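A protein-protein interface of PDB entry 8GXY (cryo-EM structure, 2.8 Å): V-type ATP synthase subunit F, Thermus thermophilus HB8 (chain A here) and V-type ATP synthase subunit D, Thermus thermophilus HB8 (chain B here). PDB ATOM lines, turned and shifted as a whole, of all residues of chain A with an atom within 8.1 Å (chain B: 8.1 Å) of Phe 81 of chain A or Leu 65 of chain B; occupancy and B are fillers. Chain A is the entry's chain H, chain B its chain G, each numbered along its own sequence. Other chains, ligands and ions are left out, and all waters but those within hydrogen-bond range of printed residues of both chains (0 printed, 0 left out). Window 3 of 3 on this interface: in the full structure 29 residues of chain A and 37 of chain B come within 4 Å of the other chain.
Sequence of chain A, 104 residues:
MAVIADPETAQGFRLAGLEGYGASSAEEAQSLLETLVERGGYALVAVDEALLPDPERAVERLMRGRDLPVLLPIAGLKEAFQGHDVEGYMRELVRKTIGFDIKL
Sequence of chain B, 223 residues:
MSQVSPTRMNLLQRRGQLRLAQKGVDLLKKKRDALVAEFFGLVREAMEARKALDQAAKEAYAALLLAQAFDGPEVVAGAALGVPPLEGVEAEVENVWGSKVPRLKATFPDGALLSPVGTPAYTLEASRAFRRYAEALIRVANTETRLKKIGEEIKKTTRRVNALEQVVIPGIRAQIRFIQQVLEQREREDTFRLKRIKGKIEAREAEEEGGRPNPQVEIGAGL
Leu 64 of chain B touches Glu 8 of chain A (CD2 to O, 2.9 Å). Leu 77 of chain A touches Tyr 61 of chain B (CD1 to CG, 3.4 Å). Lys 58 of chain B touches Ala 80 of chain A. Tyr 61 of chain B touches Phe 81 of chain A (CD2 to CE2, 3.2 Å). CD1 of Leu 65 of chain B touches CE2 of Phe 81 of chain A, 3.4 Å away. His 84 of chain A touches Asp 54 of chain B (CE1 to OD1, 3.3 Å).
O of Pro 73 of chain B is in hydrogen-bond range of NE2 of Gln 68 of chain B, at 3.3 Å.
Hydrophobic or aromatic side chains of chain A that line the printed part of chain B: Leu 77, Phe 81 and His 84. Among the printed residues, no Asp or Glu carboxylate lies within 4 Å of a Lys or Arg side-chain nitrogen of the other chain.
OH of Tyr 61 of chain B sits close to OE1 of Glu 8 of chain A (2.3 Å). The side-chain amide nitrogen (NE2) of Gln 68 of chain B sits close to the side-chain amide nitrogen (NE2) of Gln 11 of chain A, at 3.0 Å.
Of chain B, only Tyr 61 (3.2 Å) and Leu 65 (3.4 Å) come within 4 Å of Phe 81 of chain A. Leu 65 of chain B touches just one residue of chain A: Phe 81 (3.4 Å). Of the printed residues of chain B, Gln 11 of chain A touches Gln 68. Of the printed residues of chain A, Leu 64 of chain B touches Glu 8. Gln 82 of chain A touches none of the printed residues of chain B. The nearest residue of chain B that does not touch Phe 81 of chain A is Ala 62 of chain B (4.2 Å). The nearest residue of chain A that does not touch Leu 65 of chain B is Glu 8 of chain A (4.5 Å).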
ATOM      1  N   GLU A   8      11.001  10.226   1.516  1.00  0.00           N
ATOM      2  CA  GLU A   8       9.939  10.297   2.514  1.00  0.00           C
ATOM      3  C   GLU A   8      10.303   9.499   3.761  1.00  0.00           C
ATOM      4  O   GLU A   8      10.121   9.972   4.888  1.00  0.00           O
ATOM      5  CB  GLU A   8       8.625   9.801   1.912  1.00  0.00           C
ATOM      6  CG  GLU A   8       8.022  10.759   0.897  1.00  0.00           C
ATOM      7  CD  GLU A   8       6.640  10.338   0.440  1.00  0.00           C
ATOM      8  OE1 GLU A   8       6.376   9.119   0.389  1.00  0.00           O
ATOM      9  OE2 GLU A   8       5.818  11.227   0.134  1.00  0.00           O
ATOM     10  N   GLN A  11      13.846  11.015   5.393  1.00  0.00           N
ATOM     11  CA  GLN A  11      13.685  12.160   6.276  1.00  0.00           C
ATOM     12  C   GLN A  11      13.075  11.755   7.610  1.00  0.00           C
ATOM     13  O   GLN A  11      13.438  12.315   8.647  1.00  0.00           O
ATOM     14  CB  GLN A  11      12.840  13.228   5.584  1.00  0.00           C
ATOM     15  CG  GLN A  11      11.400  12.819   5.362  1.00  0.00           C
ATOM     16  CD  GLN A  11      10.652  13.778   4.461  1.00  0.00           C
ATOM     17  OE1 GLN A  11      11.245  14.669   3.851  1.00  0.00           O
ATOM     18  NE2 GLN A  11       9.344  13.586   4.351  1.00  0.00           N
ATOM     19  N   GLY A  76      10.132  -1.551   0.650  1.00  0.00           N
ATOM     20  CA  GLY A  76       9.805  -0.454  -0.243  1.00  0.00           C
ATOM     21  C   GLY A  76       8.492   0.203   0.154  1.00  0.00           C
ATOM     22  O   GLY A  76       7.495  -0.462   0.437  1.00  0.00           O
ATOM     23  N   LEU A  77       8.502   1.536   0.166  1.00  0.00           N
ATOM     24  CA  LEU A  77       7.331   2.273   0.623  1.00  0.00           C
ATOM     25  C   LEU A  77       6.140   2.044  -0.298  1.00  0.00           C
ATOM     26  O   LEU A  77       5.001   1.932   0.168  1.00  0.00           O
ATOM     27  CB  LEU A  77       7.659   3.761   0.723  1.00  0.00           C
ATOM     28  CG  LEU A  77       8.381   4.185   2.005  1.00  0.00           C
ATOM     29  CD1 LEU A  77       7.565   3.827   3.234  1.00  0.00           C
ATOM     30  CD2 LEU A  77       9.762   3.550   2.081  1.00  0.00           C
ATOM     31  N   LYS A  78       6.381   1.971  -1.607  1.00  0.00           N
ATOM     32  CA  LYS A  78       5.286   1.714  -2.537  1.00  0.00           C
ATOM     33  C   LYS A  78       4.542   0.439  -2.165  1.00  0.00           C
ATOM     34  O   LYS A  78       3.306   0.413  -2.151  1.00  0.00           O
ATOM     35  CB  LYS A  78       5.821   1.625  -3.966  1.00  0.00           C
ATOM     36  CG  LYS A  78       5.858   2.956  -4.699  1.00  0.00           C
ATOM     37  CD  LYS A  78       6.777   3.948  -4.008  1.00  0.00           C
ATOM     38  CE  LYS A  78       7.040   5.164  -4.881  1.00  0.00           C
ATOM     39  NZ  LYS A  78       7.772   6.230  -4.146  1.00  0.00           N
ATOM     40  N   GLU A  79       5.276  -0.627  -1.853  1.00  0.00           N
ATOM     41  CA  GLU A  79       4.653  -1.872  -1.427  1.00  0.00           C
ATOM     42  C   GLU A  79       4.215  -1.840   0.029  1.00  0.00           C
ATOM     43  O   GLU A  79       3.566  -2.788   0.482  1.00  0.00           O
ATOM     44  CB  GLU A  79       5.614  -3.046  -1.639  1.00  0.00           C
ATOM     45  CG  GLU A  79       5.875  -3.384  -3.100  1.00  0.00           C
ATOM     46  CD  GLU A  79       6.775  -2.376  -3.787  1.00  0.00           C
ATOM     47  OE1 GLU A  79       7.468  -1.614  -3.080  1.00  0.00           O
ATOM     48  OE2 GLU A  79       6.789  -2.344  -5.036  1.00  0.00           O
ATOM     49  N   ALA A  80       4.545  -0.779   0.764  1.00  0.00           N
ATOM     50  CA  ALA A  80       4.270  -0.763   2.195  1.00  0.00           C
ATOM     51  C   ALA A  80       2.778  -0.867   2.475  1.00  0.00           C
ATOM     52  O   ALA A  80       2.366  -1.523   3.439  1.00  0.00           O
ATOM     53  CB  ALA A  80       4.844   0.504   2.825  1.00  0.00           C
ATOM     54  N   PHE A  81       1.951  -0.225   1.652  1.00  0.00           N
ATOM     55  CA  PHE A  81       0.516  -0.177   1.886  1.00  0.00           C
ATOM     56  C   PHE A  81      -0.263  -1.175   1.040  1.00  0.00           C
ATOM     57  O   PHE A  81      -1.498  -1.158   1.066  1.00  0.00           O
ATOM     58  CB  PHE A  81      -0.008   1.239   1.638  1.00  0.00           C
ATOM     59  CG  PHE A  81       0.430   2.237   2.672  1.00  0.00           C
ATOM     60  CD1 PHE A  81       0.231   1.992   4.021  1.00  0.00           C
ATOM     61  CD2 PHE A  81       1.039   3.420   2.296  1.00  0.00           C
ATOM     62  CE1 PHE A  81       0.632   2.906   4.973  1.00  0.00           C
ATOM     63  CE2 PHE A  81       1.440   4.339   3.244  1.00  0.00           C
ATOM     64  CZ  PHE A  81       1.238   4.082   4.584  1.00  0.00           C
ATOM     65  N   GLN A  82       0.421  -2.041   0.293  1.00  0.00           N
ATOM     66  CA  GLN A  82      -0.239  -3.117  -0.432  1.00  0.00           C
ATOM     67  C   GLN A  82       0.305  -4.491  -0.075  1.00  0.00           C
ATOM     68  O   GLN A  82      -0.171  -5.492  -0.624  1.00  0.00           O
ATOM     69  CB  GLN A  82      -0.125  -2.896  -1.947  1.00  0.00           C
ATOM     70  CG  GLN A  82       1.296  -2.834  -2.468  1.00  0.00           C
ATOM     71  CD  GLN A  82       1.354  -2.738  -3.979  1.00  0.00           C
ATOM     72  OE1 GLN A  82       0.523  -2.077  -4.603  1.00  0.00           O
ATOM     73  NE2 GLN A  82       2.335  -3.402  -4.578  1.00  0.00           N
ATOM     74  N   GLY A  83       1.279  -4.571   0.819  1.00  0.00           N
ATOM     75  CA  GLY A  83       1.792  -5.857   1.259  1.00  0.00           C
ATOM     76  C   GLY A  83       2.819  -6.429   0.305  1.00  0.00           C
ATOM     77  O   GLY A  83       2.749  -6.264  -0.913  1.00  0.00           O
ATOM     78  N   HIS A  84       3.800  -7.119   0.880  1.00  0.00           N
ATOM     79  CA  HIS A  84       4.831  -7.798   0.113  1.00  0.00           C
ATOM     80  C   HIS A  84       5.027  -9.193   0.683  1.00  0.00           C
ATOM     81  O   HIS A  84       4.886  -9.414   1.889  1.00  0.00           O
ATOM     82  CB  HIS A  84       6.159  -7.034   0.137  1.00  0.00           C
ATOM     83  CG  HIS A  84       6.704  -6.815   1.513  1.00  0.00           C
ATOM     84  ND1 HIS A  84       6.413  -5.693   2.259  1.00  0.00           N
ATOM     85  CD2 HIS A  84       7.519  -7.576   2.280  1.00  0.00           C
ATOM     86  CE1 HIS A  84       7.026  -5.771   3.425  1.00  0.00           C
ATOM     87  NE2 HIS A  84       7.704  -6.904   3.465  1.00  0.00           N
ATOM     88  N   ASP B  54       7.688  -5.118   9.214  1.00  0.00           N
ATOM     89  CA  ASP B  54       6.671  -4.631   8.288  1.00  0.00           C
ATOM     90  C   ASP B  54       5.587  -3.860   9.028  1.00  0.00           C
ATOM     91  O   ASP B  54       5.168  -2.779   8.595  1.00  0.00           O
ATOM     92  CB  ASP B  54       6.066  -5.802   7.516  1.00  0.00           C
ATOM     93  CG  ASP B  54       4.979  -5.365   6.553  1.00  0.00           C
ATOM     94  OD1 ASP B  54       5.221  -4.420   5.773  1.00  0.00           O
ATOM     95  OD2 ASP B  54       3.883  -5.963   6.580  1.00  0.00           O
ATOM     96  N   ALA B  57       7.040  -0.527  10.179  1.00  0.00           N
ATOM     97  CA  ALA B  57       7.210   0.365   9.042  1.00  0.00           C
ATOM     98  C   ALA B  57       5.880   0.961   8.622  1.00  0.00           C
ATOM     99  O   ALA B  57       5.782   2.165   8.368  1.00  0.00           O
ATOM    100  CB  ALA B  57       7.839  -0.391   7.873  1.00  0.00           C
ATOM    101  N   LYS B  58       4.841   0.132   8.538  1.00  0.00           N
ATOM    102  CA  LYS B  58       3.530   0.647   8.173  1.00  0.00           C
ATOM    103  C   LYS B  58       3.085   1.717   9.157  1.00  0.00           C
ATOM    104  O   LYS B  58       2.654   2.805   8.758  1.00  0.00           O
ATOM    105  CB  LYS B  58       2.515  -0.493   8.113  1.00  0.00           C
ATOM    106  CG  LYS B  58       2.582  -1.302   6.826  1.00  0.00           C
ATOM    107  CD  LYS B  58       1.236  -1.912   6.468  1.00  0.00           C
ATOM    108  CE  LYS B  58       0.652  -2.695   7.630  1.00  0.00           C
ATOM    109  NZ  LYS B  58      -0.096  -3.896   7.167  1.00  0.00           N
ATOM    110  N   GLU B  59       3.212   1.434  10.455  1.00  0.00           N
ATOM    111  CA  GLU B  59       2.758   2.398  11.453  1.00  0.00           C
ATOM    112  C   GLU B  59       3.538   3.703  11.361  1.00  0.00           C
ATOM    113  O   GLU B  59       2.949   4.791  11.372  1.00  0.00           O
ATOM    114  CB  GLU B  59       2.880   1.799  12.852  1.00  0.00           C
ATOM    115  CG  GLU B  59       2.308   2.680  13.946  1.00  0.00           C
ATOM    116  CD  GLU B  59       2.295   1.996  15.299  1.00  0.00           C
ATOM    117  OE1 GLU B  59       2.772   0.845  15.390  1.00  0.00           O
ATOM    118  OE2 GLU B  59       1.808   2.611  16.271  1.00  0.00           O
ATOM    119  N   ALA B  60       4.865   3.619  11.256  1.00  0.00           N
ATOM    120  CA  ALA B  60       5.679   4.829  11.259  1.00  0.00           C
ATOM    121  C   ALA B  60       5.456   5.648   9.997  1.00  0.00           C
ATOM    122  O   ALA B  60       5.385   6.881  10.053  1.00  0.00           O
ATOM    123  CB  ALA B  60       7.155   4.466  11.409  1.00  0.00           C
ATOM    124  N   TYR B  61       5.352   4.985   8.848  1.00  0.00           N
ATOM    125  CA  TYR B  61       5.117   5.708   7.609  1.00  0.00           C
ATOM    126  C   TYR B  61       3.736   6.344   7.605  1.00  0.00           C
ATOM    127  O   TYR B  61       3.559   7.450   7.088  1.00  0.00           O
ATOM    128  CB  TYR B  61       5.285   4.766   6.421  1.00  0.00           C
ATOM    129  CG  TYR B  61       5.271   5.460   5.078  1.00  0.00           C
ATOM    130  CD1 TYR B  61       6.050   6.587   4.848  1.00  0.00           C
ATOM    131  CD2 TYR B  61       4.487   4.983   4.039  1.00  0.00           C
ATOM    132  CE1 TYR B  61       6.041   7.221   3.621  1.00  0.00           C
ATOM    133  CE2 TYR B  61       4.474   5.608   2.809  1.00  0.00           C
ATOM    134  CZ  TYR B  61       5.252   6.727   2.605  1.00  0.00           C
ATOM    135  OH  TYR B  61       5.240   7.354   1.382  1.00  0.00           O
ATOM    136  N   ALA B  62       2.739   5.660   8.175  1.00  0.00           N
ATOM    137  CA  ALA B  62       1.420   6.265   8.306  1.00  0.00           C
ATOM    138  C   ALA B  62       1.475   7.492   9.201  1.00  0.00           C
ATOM    139  O   ALA B  62       0.842   8.513   8.910  1.00  0.00           O
ATOM    140  CB  ALA B  62       0.428   5.243   8.860  1.00  0.00           C
ATOM    141  N   ALA B  63       2.224   7.410  10.299  1.00  0.00           N
ATOM    142  CA  ALA B  63       2.367   8.570  11.170  1.00  0.00           C
ATOM    143  C   ALA B  63       3.010   9.733  10.427  1.00  0.00           C
ATOM    144  O   ALA B  63       2.560  10.878  10.541  1.00  0.00           O
ATOM    145  CB  ALA B  63       3.188   8.200  12.404  1.00  0.00           C
ATOM    146  N   LEU B  64       4.066   9.457   9.658  1.00  0.00           N
ATOM    147  CA  LEU B  64       4.752  10.531   8.948  1.00  0.00           C
ATOM    148  C   LEU B  64       3.868  11.140   7.870  1.00  0.00           C
ATOM    149  O   LEU B  64       3.833  12.366   7.710  1.00  0.00           O
ATOM    150  CB  LEU B  64       6.049  10.019   8.331  1.00  0.00           C
ATOM    151  CG  LEU B  64       6.786  11.023   7.437  1.00  0.00           C
ATOM    152  CD1 LEU B  64       7.102  12.308   8.191  1.00  0.00           C
ATOM    153  CD2 LEU B  64       8.061  10.410   6.885  1.00  0.00           C
ATOM    154  N   LEU B  65       3.164  10.307   7.106  1.00  0.00           N
ATOM    155  CA  LEU B  65       2.291  10.836   6.065  1.00  0.00           C
ATOM    156  C   LEU B  65       1.253  11.772   6.663  1.00  0.00           C
ATOM    157  O   LEU B  65       1.078  12.906   6.200  1.00  0.00           O
ATOM    158  CB  LEU B  65       1.615   9.688   5.315  1.00  0.00           C
ATOM    159  CG  LEU B  65       2.504   8.908   4.345  1.00  0.00           C
ATOM    160  CD1 LEU B  65       1.827   7.608   3.941  1.00  0.00           C
ATOM    161  CD2 LEU B  65       2.840   9.746   3.120  1.00  0.00           C
ATOM    162  N   LEU B  66       0.566  11.321   7.714  1.00  0.00           N
ATOM    163  CA  LEU B  66      -0.373  12.184   8.413  1.00  0.00           C
ATOM    164  C   LEU B  66       0.318  13.351   9.098  1.00  0.00           C
ATOM    165  O   LEU B  66      -0.344  14.349   9.400  1.00  0.00           O
ATOM    166  CB  LEU B  66      -1.167  11.373   9.441  1.00  0.00           C
ATOM    167  CG  LEU B  66      -2.092  10.296   8.866  1.00  0.00           C
ATOM    168  CD1 LEU B  66      -2.719   9.479   9.984  1.00  0.00           C
ATOM    169  CD2 LEU B  66      -3.170  10.914   7.984  1.00  0.00           C
ATOM    170  N   ALA B  67       1.623  13.252   9.354  1.00  0.00           N
ATOM    171  CA  ALA B  67       2.358  14.410   9.846  1.00  0.00           C
ATOM    172  C   ALA B  67       2.464  15.474   8.763  1.00  0.00           C
ATOM    173  O   ALA B  67       2.302  16.668   9.034  1.00  0.00           O
ATOM    174  CB  ALA B  67       3.745  13.991  10.331  1.00  0.00           C
ATOM    175  N   GLN B  68       2.722  15.057   7.525  1.00  0.00           N
ATOM    176  CA  GLN B  68       2.813  15.984   6.407  1.00  0.00           C
ATOM    177  C   GLN B  68       1.460  16.306   5.791  1.00  0.00           C
ATOM    178  O   GLN B  68       1.390  17.171   4.912  1.00  0.00           O
ATOM    179  CB  GLN B  68       3.737  15.419   5.328  1.00  0.00           C
ATOM    180  CG  GLN B  68       5.195  15.387   5.727  1.00  0.00           C
ATOM    181  CD  GLN B  68       6.111  15.155   4.546  1.00  0.00           C
ATOM    182  OE1 GLN B  68       5.748  14.476   3.585  1.00  0.00           O
ATOM    183  NE2 GLN B  68       7.302  15.739   4.602  1.00  0.00           N
ATOM    184  N   ALA B  69       0.392  15.632   6.219  1.00  0.00           N
ATOM    185  CA  ALA B  69      -0.948  15.950   5.743  1.00  0.00           C
ATOM    186  C   ALA B  69      -1.601  17.023   6.607  1.00  0.00           C
ATOM    187  O   ALA B  69      -2.133  18.006   6.083  1.00  0.00           O
ATOM    188  CB  ALA B  69      -1.814  14.686   5.720  1.00  0.00           C
ATOM    189  N   PHE B  70      -1.565  16.848   7.929  1.00  0.00           N
ATOM    190  CA  PHE B  70      -2.126  17.857   8.821  1.00  0.00           C
ATOM    191  C   PHE B  70      -1.256  19.107   8.866  1.00  0.00           C
ATOM    192  O   PHE B  70      -1.777  20.215   9.036  1.00  0.00           O
ATOM    193  CB  PHE B  70      -2.301  17.275  10.222  1.00  0.00           C
ATOM    194  CG  PHE B  70      -3.451  16.315  10.336  1.00  0.00           C
ATOM    195  CD1 PHE B  70      -4.755  16.750  10.169  1.00  0.00           C
ATOM    196  CD2 PHE B  70      -3.228  14.974  10.606  1.00  0.00           C
ATOM    197  CE1 PHE B  70      -5.815  15.869  10.270  1.00  0.00           C
ATOM    198  CE2 PHE B  70      -4.285  14.089  10.709  1.00  0.00           C
ATOM    199  CZ  PHE B  70      -5.579  14.537  10.540  1.00  0.00           C
ATOM    200  N   ASP B  71       0.055  18.952   8.715  1.00  0.00           N
ATOM    201  CA  ASP B  71       0.976  20.072   8.607  1.00  0.00           C
ATOM    202  C   ASP B  71       1.533  20.123   7.190  1.00  0.00           C
ATOM    203  O   ASP B  71       1.609  19.104   6.499  1.00  0.00           O
ATOM    204  CB  ASP B  71       2.124  19.949   9.618  1.00  0.00           C
ATOM    205  CG  ASP B  71       3.202  21.008   9.421  1.00  0.00           C
ATOM    206  OD1 ASP B  71       3.044  21.885   8.546  1.00  0.00           O
ATOM    207  OD2 ASP B  71       4.221  20.960  10.140  1.00  0.00           O
ATOM    208  N   PRO B  73       3.780  19.930   4.107  1.00  0.00           N
ATOM    209  CA  PRO B  73       4.912  19.011   3.896  1.00  0.00           C
ATOM    210  C   PRO B  73       6.267  19.680   4.042  1.00  0.00           C
ATOM    211  O   PRO B  73       7.198  19.068   4.579  1.00  0.00           O
ATOM    212  CB  PRO B  73       4.686  18.498   2.467  1.00  0.00           C
ATOM    213  CG  PRO B  73       3.234  18.667   2.222  1.00  0.00           C
ATOM    214  CD  PRO B  73       2.827  19.891   2.982  1.00  0.00           C
ATOM    215  N   VAL B  76       7.204  20.161   7.815  1.00  0.00           N
ATOM    216  CA  VAL B  76       7.481  18.879   8.453  1.00  0.00           C
ATOM    217  C   VAL B  76       8.819  18.332   7.979  1.00  0.00           C
ATOM    218  O   VAL B  76       9.615  17.817   8.770  1.00  0.00           O
ATOM    219  CB  VAL B  76       6.340  17.886   8.173  1.00  0.00           C
ATOM    220  CG1 VAL B  76       6.692  16.495   8.696  1.00  0.00           C
ATOM    221  CG2 VAL B  76       5.044  18.386   8.779  1.00  0.00           C
ATOM    222  N   TYR B 122       2.074  16.695  15.504  1.00  0.00           N
ATOM    223  CA  TYR B 122       2.264  15.252  15.540  1.00  0.00           C
ATOM    224  C   TYR B 122       3.693  14.823  15.231  1.00  0.00           C
ATOM    225  O   TYR B 122       4.036  13.662  15.474  1.00  0.00           O
ATOM    226  CB  TYR B 122       1.313  14.582  14.546  1.00  0.00           C
ATOM    227  CG  TYR B 122       0.967  13.153  14.893  1.00  0.00           C
ATOM    228  CD1 TYR B 122      -0.047  12.862  15.795  1.00  0.00           C
ATOM    229  CD2 TYR B 122       1.653  12.093  14.315  1.00  0.00           C
ATOM    230  CE1 TYR B 122      -0.367  11.557  16.114  1.00  0.00           C
ATOM    231  CE2 TYR B 122       1.339  10.783  14.626  1.00  0.00           C
ATOM    232  CZ  TYR B 122       0.329  10.521  15.526  1.00  0.00           C
ATOM    233  OH  TYR B 122       0.013   9.220  15.839  1.00  0.00           O
ATOM    234  N   ALA B 126       5.590  11.097  15.411  1.00  0.00           N
ATOM    235  CA  ALA B 126       6.216  10.411  14.287  1.00  0.00           C
ATOM    236  C   ALA B 126       7.626   9.959  14.631  1.00  0.00           C
ATOM    237  O   ALA B 126       8.015   8.834  14.300  1.00  0.00           O
ATOM    238  CB  ALA B 126       6.237  11.319  13.060  1.00  0.00           C
ATOM    239  N   PHE B 130       9.323   6.135  14.331  1.00  0.00           N
ATOM    240  CA  PHE B 130      10.545   5.827  13.598  1.00  0.00           C
ATOM    241  C   PHE B 130      11.639   5.298  14.514  1.00  0.00           C
ATOM    242  O   PHE B 130      12.456   4.480  14.083  1.00  0.00           O
ATOM    243  CB  PHE B 130      11.041   7.055  12.840  1.00  0.00           C
ATOM    244  CG  PHE B 130      10.204   7.405  11.654  1.00  0.00           C
ATOM    245  CD1 PHE B 130      10.291   6.661  10.491  1.00  0.00           C
ATOM    246  CD2 PHE B 130       9.326   8.470  11.696  1.00  0.00           C
ATOM    247  CE1 PHE B 130       9.522   6.972   9.396  1.00  0.00           C
ATOM    248  CE2 PHE B 130       8.554   8.788  10.603  1.00  0.00           C
ATOM    249  CZ  PHE B 130       8.652   8.035   9.449  1.00  0.00           C
